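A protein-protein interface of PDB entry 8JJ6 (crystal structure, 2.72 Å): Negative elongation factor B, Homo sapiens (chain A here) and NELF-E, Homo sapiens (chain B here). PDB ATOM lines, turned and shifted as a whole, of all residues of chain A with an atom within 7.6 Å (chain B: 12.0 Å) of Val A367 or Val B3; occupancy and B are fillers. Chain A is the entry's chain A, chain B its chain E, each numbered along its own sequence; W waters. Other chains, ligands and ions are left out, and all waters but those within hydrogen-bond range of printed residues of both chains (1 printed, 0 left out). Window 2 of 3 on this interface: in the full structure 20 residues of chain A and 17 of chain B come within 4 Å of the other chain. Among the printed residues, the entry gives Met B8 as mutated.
Arg A333 touches Ile B4 (NH2 to CG2, 3.0 Å).
Pro B6 touches Arg A333 (O to NH2, 3.8 Å).
NH1 of Arg A333 touches O of Gly B7 (3.6 Å).
Val A367 touches Val B3 (CG2 to O, 3.3 Å).
CA of Thr A371 touches OE2 of Glu B12, 3.5 Å away.
Water W1 lies within hydrogen-bond range of N of Arg A333 (2.6 Å), O of Ile A370 (2.9 Å) and OE2 of Glu B12 (3.2 Å).
Of the printed residues of chain B, Val A367 touches Val B3 (3.3 Å).
Printed residues of chain A within 4 Å of Val B3: Val A367 (3.3 Å).
No residue of chain B comes within 4 Å of Glu A368.
No residue of chain B comes within 4 Å of Leu A369.
No residue of chain B comes within 4 Å of Ile A370.
Thr A371 touches just these residues of chain B: Ser B9 (2.9 Å) and Glu B12 (3.5 Å).
Of the printed residues of chain A, Glu B11 touches Arg A372 (3.2 Å).
Printed residues of chain A within 4 Å of Pro B6: Arg A333.
Of the printed residues of chain B, Arg A372 touches Glu B11.
Of the printed residues of chain A, Gly B7 touches Arg A333.
The nearest residue of chain B that does not touch Val A367 is Pro B5 (4.2 Å).
The nearest printed residue of chain B that does not touch Arg A372 is Ser B9 (4.1 Å).
O of Val A367 is in hydrogen-bond range of OG1 of Thr A371.
NH1 of Arg A372 lies within salt-bridge range of OE2 of Glu A368, at 3.7 Å.
The side-chain carboxylate (OE1) of Glu B11 sits at hydrogen-bond distance from the side-chain hydroxyl (OG) of Ser B9 (3.2 Å).
The backbone NH of Ser B9 lies within hydrogen-bond range of the side-chain carboxylate of Glu B12 (2.7 Å).
Of the 14 printed residues of chain A, 4 touch a printed residue of chain B.
Of the 11 printed residues of chain B, 8 touch a printed residue of chain A.
Printed residues of chain B that touch a printed residue of chain A: Val B3, Ile B4, Pro B5, Pro B6, Gly B7, Ser B9, Glu B11 and Glu B12.
Hydrophobic or aromatic side chains of chain B that line the printed part of chain A: Ile B4.
Among the printed residues, 9 pairs touch across the chains.
The backbone carbonyl oxygen (O) of Pro B5 sits close to the guanidinium group (NH2) of Arg A333, 2.3 Å away.
The guanidinium group of Arg A333 lies within salt-bridge range of the side-chain carboxylate of Glu B12 (2.7 Å).
The side-chain carboxylate (OE2) of Glu B11 lies within salt-bridge range of the guanidinium group (NE) of Arg A372, 3.2 Å away.
The backbone carbonyl oxygen of Thr A371 lies within hydrogen-bond range of the side-chain hydroxyl of Ser B9 (2.9 Å).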
ATOM      1  N   ARG A 333      -3.166  -6.403   9.169  1.00  0.00           N
ATOM      2  CA  ARG A 333      -3.895  -5.471   8.325  1.00  0.00           C
ATOM      3  C   ARG A 333      -4.601  -6.185   7.179  1.00  0.00           C
ATOM      4  O   ARG A 333      -5.574  -5.667   6.626  1.00  0.00           O
ATOM      5  CB  ARG A 333      -2.928  -4.419   7.782  1.00  0.00           C
ATOM      6  CG  ARG A 333      -1.911  -4.977   6.792  1.00  0.00           C
ATOM      7  CD  ARG A 333      -0.706  -4.108   6.707  1.00  0.00           C
ATOM      8  NE  ARG A 333      -0.966  -2.828   6.056  1.00  0.00           N
ATOM      9  CZ  ARG A 333      -0.230  -1.730   6.251  1.00  0.00           C
ATOM     10  NH1 ARG A 333       0.793  -1.740   7.107  1.00  0.00           N
ATOM     11  NH2 ARG A 333      -0.519  -0.611   5.593  1.00  0.00           N
ATOM     12  N   LYS A 364     -13.172   5.082  17.964  1.00  0.00           N
ATOM     13  CA  LYS A 364     -12.147   5.163  16.939  1.00  0.00           C
ATOM     14  C   LYS A 364     -11.217   3.961  17.046  1.00  0.00           C
ATOM     15  O   LYS A 364     -10.726   3.638  18.129  1.00  0.00           O
ATOM     16  CB  LYS A 364     -11.362   6.466  17.093  1.00  0.00           C
ATOM     17  CG  LYS A 364     -10.379   6.728  15.942  1.00  0.00           C
ATOM     18  CD  LYS A 364      -9.326   7.787  16.298  1.00  0.00           C
ATOM     19  CE  LYS A 364      -9.912   9.198  16.299  1.00  0.00           C
ATOM     20  NZ  LYS A 364      -9.161  10.086  17.237  1.00  0.00           N
ATOM     21  N   MET A 365     -10.986   3.286  15.921  1.00  0.00           N
ATOM     22  CA  MET A 365     -10.023   2.190  15.874  1.00  0.00           C
ATOM     23  C   MET A 365      -8.611   2.729  15.656  1.00  0.00           C
ATOM     24  O   MET A 365      -8.341   3.399  14.652  1.00  0.00           O
ATOM     25  CB  MET A 365     -10.374   1.214  14.761  1.00  0.00           C
ATOM     26  CG  MET A 365      -9.302   0.162  14.561  1.00  0.00           C
ATOM     27  SD  MET A 365      -9.476  -1.149  15.780  1.00  0.00           S
ATOM     28  CE  MET A 365     -10.782  -2.122  15.027  1.00  0.00           C
ATOM     29  N   GLU A 366      -7.704   2.418  16.577  1.00  0.00           N
ATOM     30  CA  GLU A 366      -6.326   2.899  16.498  1.00  0.00           C
ATOM     31  C   GLU A 366      -5.560   2.126  15.420  1.00  0.00           C
ATOM     32  O   GLU A 366      -5.327   0.916  15.547  1.00  0.00           O
ATOM     33  CB  GLU A 366      -5.648   2.774  17.859  1.00  0.00           C
ATOM     34  CG  GLU A 366      -4.545   3.792  18.093  1.00  0.00           C
ATOM     35  CD  GLU A 366      -5.066   5.119  18.635  1.00  0.00           C
ATOM     36  OE1 GLU A 366      -6.112   5.104  19.323  1.00  0.00           O
ATOM     37  OE2 GLU A 366      -4.427   6.173  18.372  1.00  0.00           O
ATOM     38  N   VAL A 367      -5.180   2.838  14.356  1.00  0.00           N
ATOM     39  CA  VAL A 367      -4.362   2.296  13.268  1.00  0.00           C
ATOM     40  C   VAL A 367      -3.140   1.551  13.802  1.00  0.00           C
ATOM     41  O   VAL A 367      -2.776   0.476  13.304  1.00  0.00           O
ATOM     42  CB  VAL A 367      -3.941   3.445  12.323  1.00  0.00           C
ATOM     43  CG1 VAL A 367      -2.837   3.009  11.366  1.00  0.00           C
ATOM     44  CG2 VAL A 367      -5.139   3.967  11.547  1.00  0.00           C
ATOM     45  N   GLU A 368      -2.464   2.119  14.799  1.00  0.00           N
ATOM     46  CA  GLU A 368      -1.198   1.522  15.199  1.00  0.00           C
ATOM     47  C   GLU A 368      -1.376   0.201  15.937  1.00  0.00           C
ATOM     48  O   GLU A 368      -0.435  -0.594  15.980  1.00  0.00           O
ATOM     49  CB  GLU A 368      -0.392   2.512  16.027  1.00  0.00           C
ATOM     50  CG  GLU A 368       0.298   3.567  15.151  1.00  0.00           C
ATOM     51  CD  GLU A 368       1.257   4.454  15.919  1.00  0.00           C
ATOM     52  OE1 GLU A 368       2.174   5.014  15.284  1.00  0.00           O
ATOM     53  OE2 GLU A 368       1.098   4.586  17.152  1.00  0.00           O
ATOM     54  N   LEU A 369      -2.551  -0.057  16.508  1.00  0.00           N
ATOM     55  CA  LEU A 369      -2.786  -1.348  17.136  1.00  0.00           C
ATOM     56  C   LEU A 369      -2.777  -2.458  16.099  1.00  0.00           C
ATOM     57  O   LEU A 369      -2.397  -3.594  16.398  1.00  0.00           O
ATOM     58  CB  LEU A 369      -4.121  -1.329  17.889  1.00  0.00           C
ATOM     59  CG  LEU A 369      -4.556  -2.716  18.413  1.00  0.00           C
ATOM     60  CD1 LEU A 369      -3.945  -2.994  19.759  1.00  0.00           C
ATOM     61  CD2 LEU A 369      -6.055  -2.937  18.472  1.00  0.00           C
ATOM     62  N   ILE A 370      -3.182  -2.148  14.873  1.00  0.00           N
ATOM     63  CA  ILE A 370      -3.200  -3.161  13.831  1.00  0.00           C
ATOM     64  C   ILE A 370      -1.839  -3.256  13.133  1.00  0.00           C
ATOM     65  O   ILE A 370      -1.406  -4.346  12.743  1.00  0.00           O
ATOM     66  CB  ILE A 370      -4.338  -2.844  12.842  1.00  0.00           C
ATOM     67  CG1 ILE A 370      -5.700  -2.929  13.530  1.00  0.00           C
ATOM     68  CG2 ILE A 370      -4.290  -3.779  11.653  1.00  0.00           C
ATOM     69  CD1 ILE A 370      -6.699  -1.911  13.021  1.00  0.00           C
ATOM     70  N   THR A 371      -1.133  -2.129  12.978  1.00  0.00           N
ATOM     71  CA  THR A 371       0.135  -2.131  12.252  1.00  0.00           C
ATOM     72  C   THR A 371       1.348  -2.327  13.150  1.00  0.00           C
ATOM     73  O   THR A 371       2.394  -2.768  12.670  1.00  0.00           O
ATOM     74  CB  THR A 371       0.332  -0.818  11.481  1.00  0.00           C
ATOM     75  OG1 THR A 371       0.383   0.280  12.406  1.00  0.00           O
ATOM     76  CG2 THR A 371      -0.780  -0.597  10.451  1.00  0.00           C
ATOM     77  N   ARG A 372       1.264  -1.985  14.427  1.00  0.00           N
ATOM     78  CA  ARG A 372       2.420  -2.117  15.304  1.00  0.00           C
ATOM     79  C   ARG A 372       2.200  -3.121  16.428  1.00  0.00           C
ATOM     80  O   ARG A 372       3.039  -4.002  16.634  1.00  0.00           O
ATOM     81  CB  ARG A 372       2.799  -0.741  15.868  1.00  0.00           C
ATOM     82  CG  ARG A 372       3.172   0.244  14.774  1.00  0.00           C
ATOM     83  CD  ARG A 372       3.306   1.698  15.253  1.00  0.00           C
ATOM     84  NE  ARG A 372       4.673   2.061  15.628  1.00  0.00           N
ATOM     85  CZ  ARG A 372       5.026   2.490  16.839  1.00  0.00           C
ATOM     86  NH1 ARG A 372       4.109   2.621  17.790  1.00  0.00           N
ATOM     87  NH2 ARG A 372       6.289   2.789  17.106  1.00  0.00           N
ATOM     88  N   PHE A 373       1.068  -3.057  17.133  1.00  0.00           N
ATOM     89  CA  PHE A 373       0.942  -3.869  18.339  1.00  0.00           C
ATOM     90  C   PHE A 373       0.691  -5.333  18.017  1.00  0.00           C
ATOM     91  O   PHE A 373       1.404  -6.214  18.512  1.00  0.00           O
ATOM     92  CB  PHE A 373      -0.178  -3.366  19.249  1.00  0.00           C
ATOM     93  CG  PHE A 373      -0.358  -4.225  20.478  1.00  0.00           C
ATOM     94  CD1 PHE A 373      -1.436  -5.112  20.589  1.00  0.00           C
ATOM     95  CD2 PHE A 373       0.581  -4.183  21.500  1.00  0.00           C
ATOM     96  CE1 PHE A 373      -1.583  -5.907  21.712  1.00  0.00           C
ATOM     97  CE2 PHE A 373       0.448  -4.970  22.621  1.00  0.00           C
ATOM     98  CZ  PHE A 373      -0.634  -5.835  22.736  1.00  0.00           C
ATOM     99  N   PRO A 375       1.318  -6.849  15.271  1.00  0.00           N
ATOM    100  CA  PRO A 375       2.542  -7.428  14.717  1.00  0.00           C
ATOM    101  C   PRO A 375       3.565  -7.826  15.768  1.00  0.00           C
ATOM    102  O   PRO A 375       4.221  -8.868  15.613  1.00  0.00           O
ATOM    103  CB  PRO A 375       3.037  -6.314  13.790  1.00  0.00           C
ATOM    104  CG  PRO A 375       1.792  -5.767  13.268  1.00  0.00           C
ATOM    105  CD  PRO A 375       0.889  -5.688  14.464  1.00  0.00           C
ATOM    106  N   PHE A 414       1.913   0.183  24.739  1.00  0.00           N
ATOM    107  CA  PHE A 414       0.554  -0.183  24.335  1.00  0.00           C
ATOM    108  C   PHE A 414      -0.195  -0.812  25.498  1.00  0.00           C
ATOM    109  O   PHE A 414      -1.369  -0.489  25.747  1.00  0.00           O
ATOM    110  CB  PHE A 414       0.561  -1.169  23.165  1.00  0.00           C
ATOM    111  CG  PHE A 414       0.642  -0.534  21.791  1.00  0.00           C
ATOM    112  CD1 PHE A 414      -0.472   0.050  21.204  1.00  0.00           C
ATOM    113  CD2 PHE A 414       1.828  -0.582  21.058  1.00  0.00           C
ATOM    114  CE1 PHE A 414      -0.402   0.602  19.927  1.00  0.00           C
ATOM    115  CE2 PHE A 414       1.901  -0.032  19.790  1.00  0.00           C
ATOM    116  CZ  PHE A 414       0.782   0.562  19.221  1.00  0.00           C
ATOM    117  N   GLN A 418      -3.701   1.453  26.336  1.00  0.00           N
ATOM    118  CA  GLN A 418      -4.765   1.089  25.407  1.00  0.00           C
ATOM    119  C   GLN A 418      -5.553  -0.118  25.906  1.00  0.00           C
ATOM    120  O   GLN A 418      -5.017  -1.235  25.970  1.00  0.00           O
ATOM    121  CB  GLN A 418      -4.184   0.807  24.029  1.00  0.00           C
ATOM    122  CG  GLN A 418      -3.917   2.055  23.263  1.00  0.00           C
ATOM    123  CD  GLN A 418      -3.882   1.827  21.775  1.00  0.00           C
ATOM    124  OE1 GLN A 418      -3.364   2.660  21.024  1.00  0.00           O
ATOM    125  NE2 GLN A 418      -4.437   0.693  21.328  1.00  0.00           N
ATOM    126  N   LEU B   2     -11.358   3.439   8.110  1.00  0.00           N
ATOM    127  CA  LEU B   2     -10.739   2.229   7.563  1.00  0.00           C
ATOM    128  C   LEU B   2      -9.379   2.534   6.937  1.00  0.00           C
ATOM    129  O   LEU B   2      -8.878   1.758   6.138  1.00  0.00           O
ATOM    130  CB  LEU B   2     -11.645   1.580   6.502  1.00  0.00           C
ATOM    131  CG  LEU B   2     -13.081   1.097   6.799  1.00  0.00           C
ATOM    132  CD1 LEU B   2     -13.226   0.483   8.187  1.00  0.00           C
ATOM    133  CD2 LEU B   2     -14.104   2.229   6.577  1.00  0.00           C
ATOM    134  N   VAL B   3      -8.787   3.664   7.296  1.00  0.00           N
ATOM    135  CA  VAL B   3      -7.672   4.219   6.536  1.00  0.00           C
ATOM    136  C   VAL B   3      -6.363   3.771   7.168  1.00  0.00           C
ATOM    137  O   VAL B   3      -6.136   3.971   8.370  1.00  0.00           O
ATOM    138  CB  VAL B   3      -7.748   5.756   6.464  1.00  0.00           C
ATOM    139  CG1 VAL B   3      -6.730   6.293   5.440  1.00  0.00           C
ATOM    140  CG2 VAL B   3      -9.122   6.221   6.075  1.00  0.00           C
ATOM    141  N   ILE B   4      -5.497   3.176   6.350  1.00  0.00           N
ATOM    142  CA  ILE B   4      -4.181   2.688   6.758  1.00  0.00           C
ATOM    143  C   ILE B   4      -3.175   3.180   5.725  1.00  0.00           C
ATOM    144  O   ILE B   4      -3.485   3.201   4.527  1.00  0.00           O
ATOM    145  CB  ILE B   4      -4.166   1.151   6.886  1.00  0.00           C
ATOM    146  CG1 ILE B   4      -5.101   0.691   8.024  1.00  0.00           C
ATOM    147  CG2 ILE B   4      -2.761   0.634   7.106  1.00  0.00           C
ATOM    148  CD1 ILE B   4      -5.003  -0.790   8.397  1.00  0.00           C
ATOM    149  N   PRO B   5      -1.989   3.626   6.125  1.00  0.00           N
ATOM    150  CA  PRO B   5      -0.945   3.947   5.127  1.00  0.00           C
ATOM    151  C   PRO B   5      -0.463   2.682   4.431  1.00  0.00           C
ATOM    152  O   PRO B   5      -0.337   1.622   5.065  1.00  0.00           O
ATOM    153  CB  PRO B   5       0.165   4.595   5.972  1.00  0.00           C
ATOM    154  CG  PRO B   5      -0.106   4.144   7.415  1.00  0.00           C
ATOM    155  CD  PRO B   5      -1.588   3.939   7.511  1.00  0.00           C
ATOM    156  N   PRO B   6      -0.192   2.739   3.123  1.00  0.00           N
ATOM    157  CA  PRO B   6       0.133   1.495   2.393  1.00  0.00           C
ATOM    158  C   PRO B   6       1.513   0.936   2.703  1.00  0.00           C
ATOM    159  O   PRO B   6       1.719  -0.280   2.577  1.00  0.00           O
ATOM    160  CB  PRO B   6       0.014   1.908   0.921  1.00  0.00           C
ATOM    161  CG  PRO B   6       0.339   3.359   0.932  1.00  0.00           C
ATOM    162  CD  PRO B   6      -0.209   3.911   2.237  1.00  0.00           C
ATOM    163  N   GLY B   7       2.462   1.778   3.098  1.00  0.00           N
ATOM    164  CA  GLY B   7       3.765   1.279   3.473  1.00  0.00           C
ATOM    165  C   GLY B   7       3.739   0.526   4.790  1.00  0.00           C
ATOM    166  O   GLY B   7       2.920   0.783   5.675  1.00  0.00           O
ATOM    167  N   MET B   8       4.676  -0.411   4.928  1.00  0.00           N
ATOM    168  CA  MET B   8       4.750  -1.234   6.123  1.00  0.00           C
ATOM    169  C   MET B   8       5.479  -0.519   7.247  1.00  0.00           C
ATOM    170  O   MET B   8       6.384   0.292   7.028  1.00  0.00           O
ATOM    171  CB  MET B   8       5.437  -2.563   5.829  1.00  0.00           C
ATOM    172  CG  MET B   8       4.427  -3.680   5.637  1.00  0.00           C
ATOM    173  SD  MET B   8       5.128  -5.053   4.750  1.00  0.00           S
ATOM    174  CE  MET B   8       6.539  -5.453   5.748  1.00  0.00           C
ATOM    175  N   SER B   9       5.052  -0.807   8.463  1.00  0.00           N
ATOM    176  CA  SER B   9       5.711  -0.230   9.612  1.00  0.00           C
ATOM    177  C   SER B   9       6.962  -1.032   9.927  1.00  0.00           C
ATOM    178  O   SER B   9       7.207  -2.100   9.368  1.00  0.00           O
ATOM    179  CB  SER B   9       4.780  -0.213  10.822  1.00  0.00           C
ATOM    180  OG  SER B   9       4.752  -1.487  11.445  1.00  0.00           O
ATOM    181  N   GLU B  10       7.752  -0.504  10.855  1.00  0.00           N
ATOM    182  CA  GLU B  10       8.929  -1.227  11.298  1.00  0.00           C
ATOM    183  C   GLU B  10       8.557  -2.596  11.841  1.00  0.00           C
ATOM    184  O   GLU B  10       9.129  -3.612  11.434  1.00  0.00           O
ATOM    185  CB  GLU B  10       9.659  -0.406  12.346  1.00  0.00           C
ATOM    186  CG  GLU B  10      10.946   0.170  11.823  1.00  0.00           C
ATOM    187  CD  GLU B  10      11.336   1.417  12.556  1.00  0.00           C
ATOM    188  OE1 GLU B  10      11.136   1.463  13.797  1.00  0.00           O
ATOM    189  OE2 GLU B  10      11.835   2.347  11.888  1.00  0.00           O
ATOM    190  N   GLU B  11       7.584  -2.640  12.756  1.00  0.00           N
ATOM    191  CA  GLU B  11       7.196  -3.898  13.384  1.00  0.00           C
ATOM    192  C   GLU B  11       6.674  -4.892  12.354  1.00  0.00           C
ATOM    193  O   GLU B  11       6.898  -6.104  12.485  1.00  0.00           O
ATOM    194  CB  GLU B  11       6.150  -3.629  14.466  1.00  0.00           C
ATOM    195  CG  GLU B  11       6.617  -2.723  15.623  1.00  0.00           C
ATOM    196  CD  GLU B  11       6.461  -1.217  15.342  1.00  0.00           C
ATOM    197  OE1 GLU B  11       6.313  -0.817  14.158  1.00  0.00           O
ATOM    198  OE2 GLU B  11       6.504  -0.420  16.316  1.00  0.00           O
ATOM    199  N   GLU B  12       5.996  -4.402  11.311  1.00  0.00           N
ATOM    200  CA  GLU B  12       5.547  -5.292  10.243  1.00  0.00           C
ATOM    201  C   GLU B  12       6.733  -5.927   9.512  1.00  0.00           C
ATOM    202  O   GLU B  12       6.796  -7.154   9.363  1.00  0.00           O
ATOM    203  CB  GLU B  12       4.638  -4.526   9.282  1.00  0.00           C
ATOM    204  CG  GLU B  12       3.167  -4.589   9.673  1.00  0.00           C
ATOM    205  CD  GLU B  12       2.329  -3.415   9.162  1.00  0.00           C
ATOM    206  OE1 GLU B  12       2.872  -2.388   8.702  1.00  0.00           O
ATOM    207  OE2 GLU B  12       1.101  -3.513   9.241  1.00  0.00           O
HETATM  208  O   HOH W   1      -0.911  -5.774  10.226  1.00  0.00           O
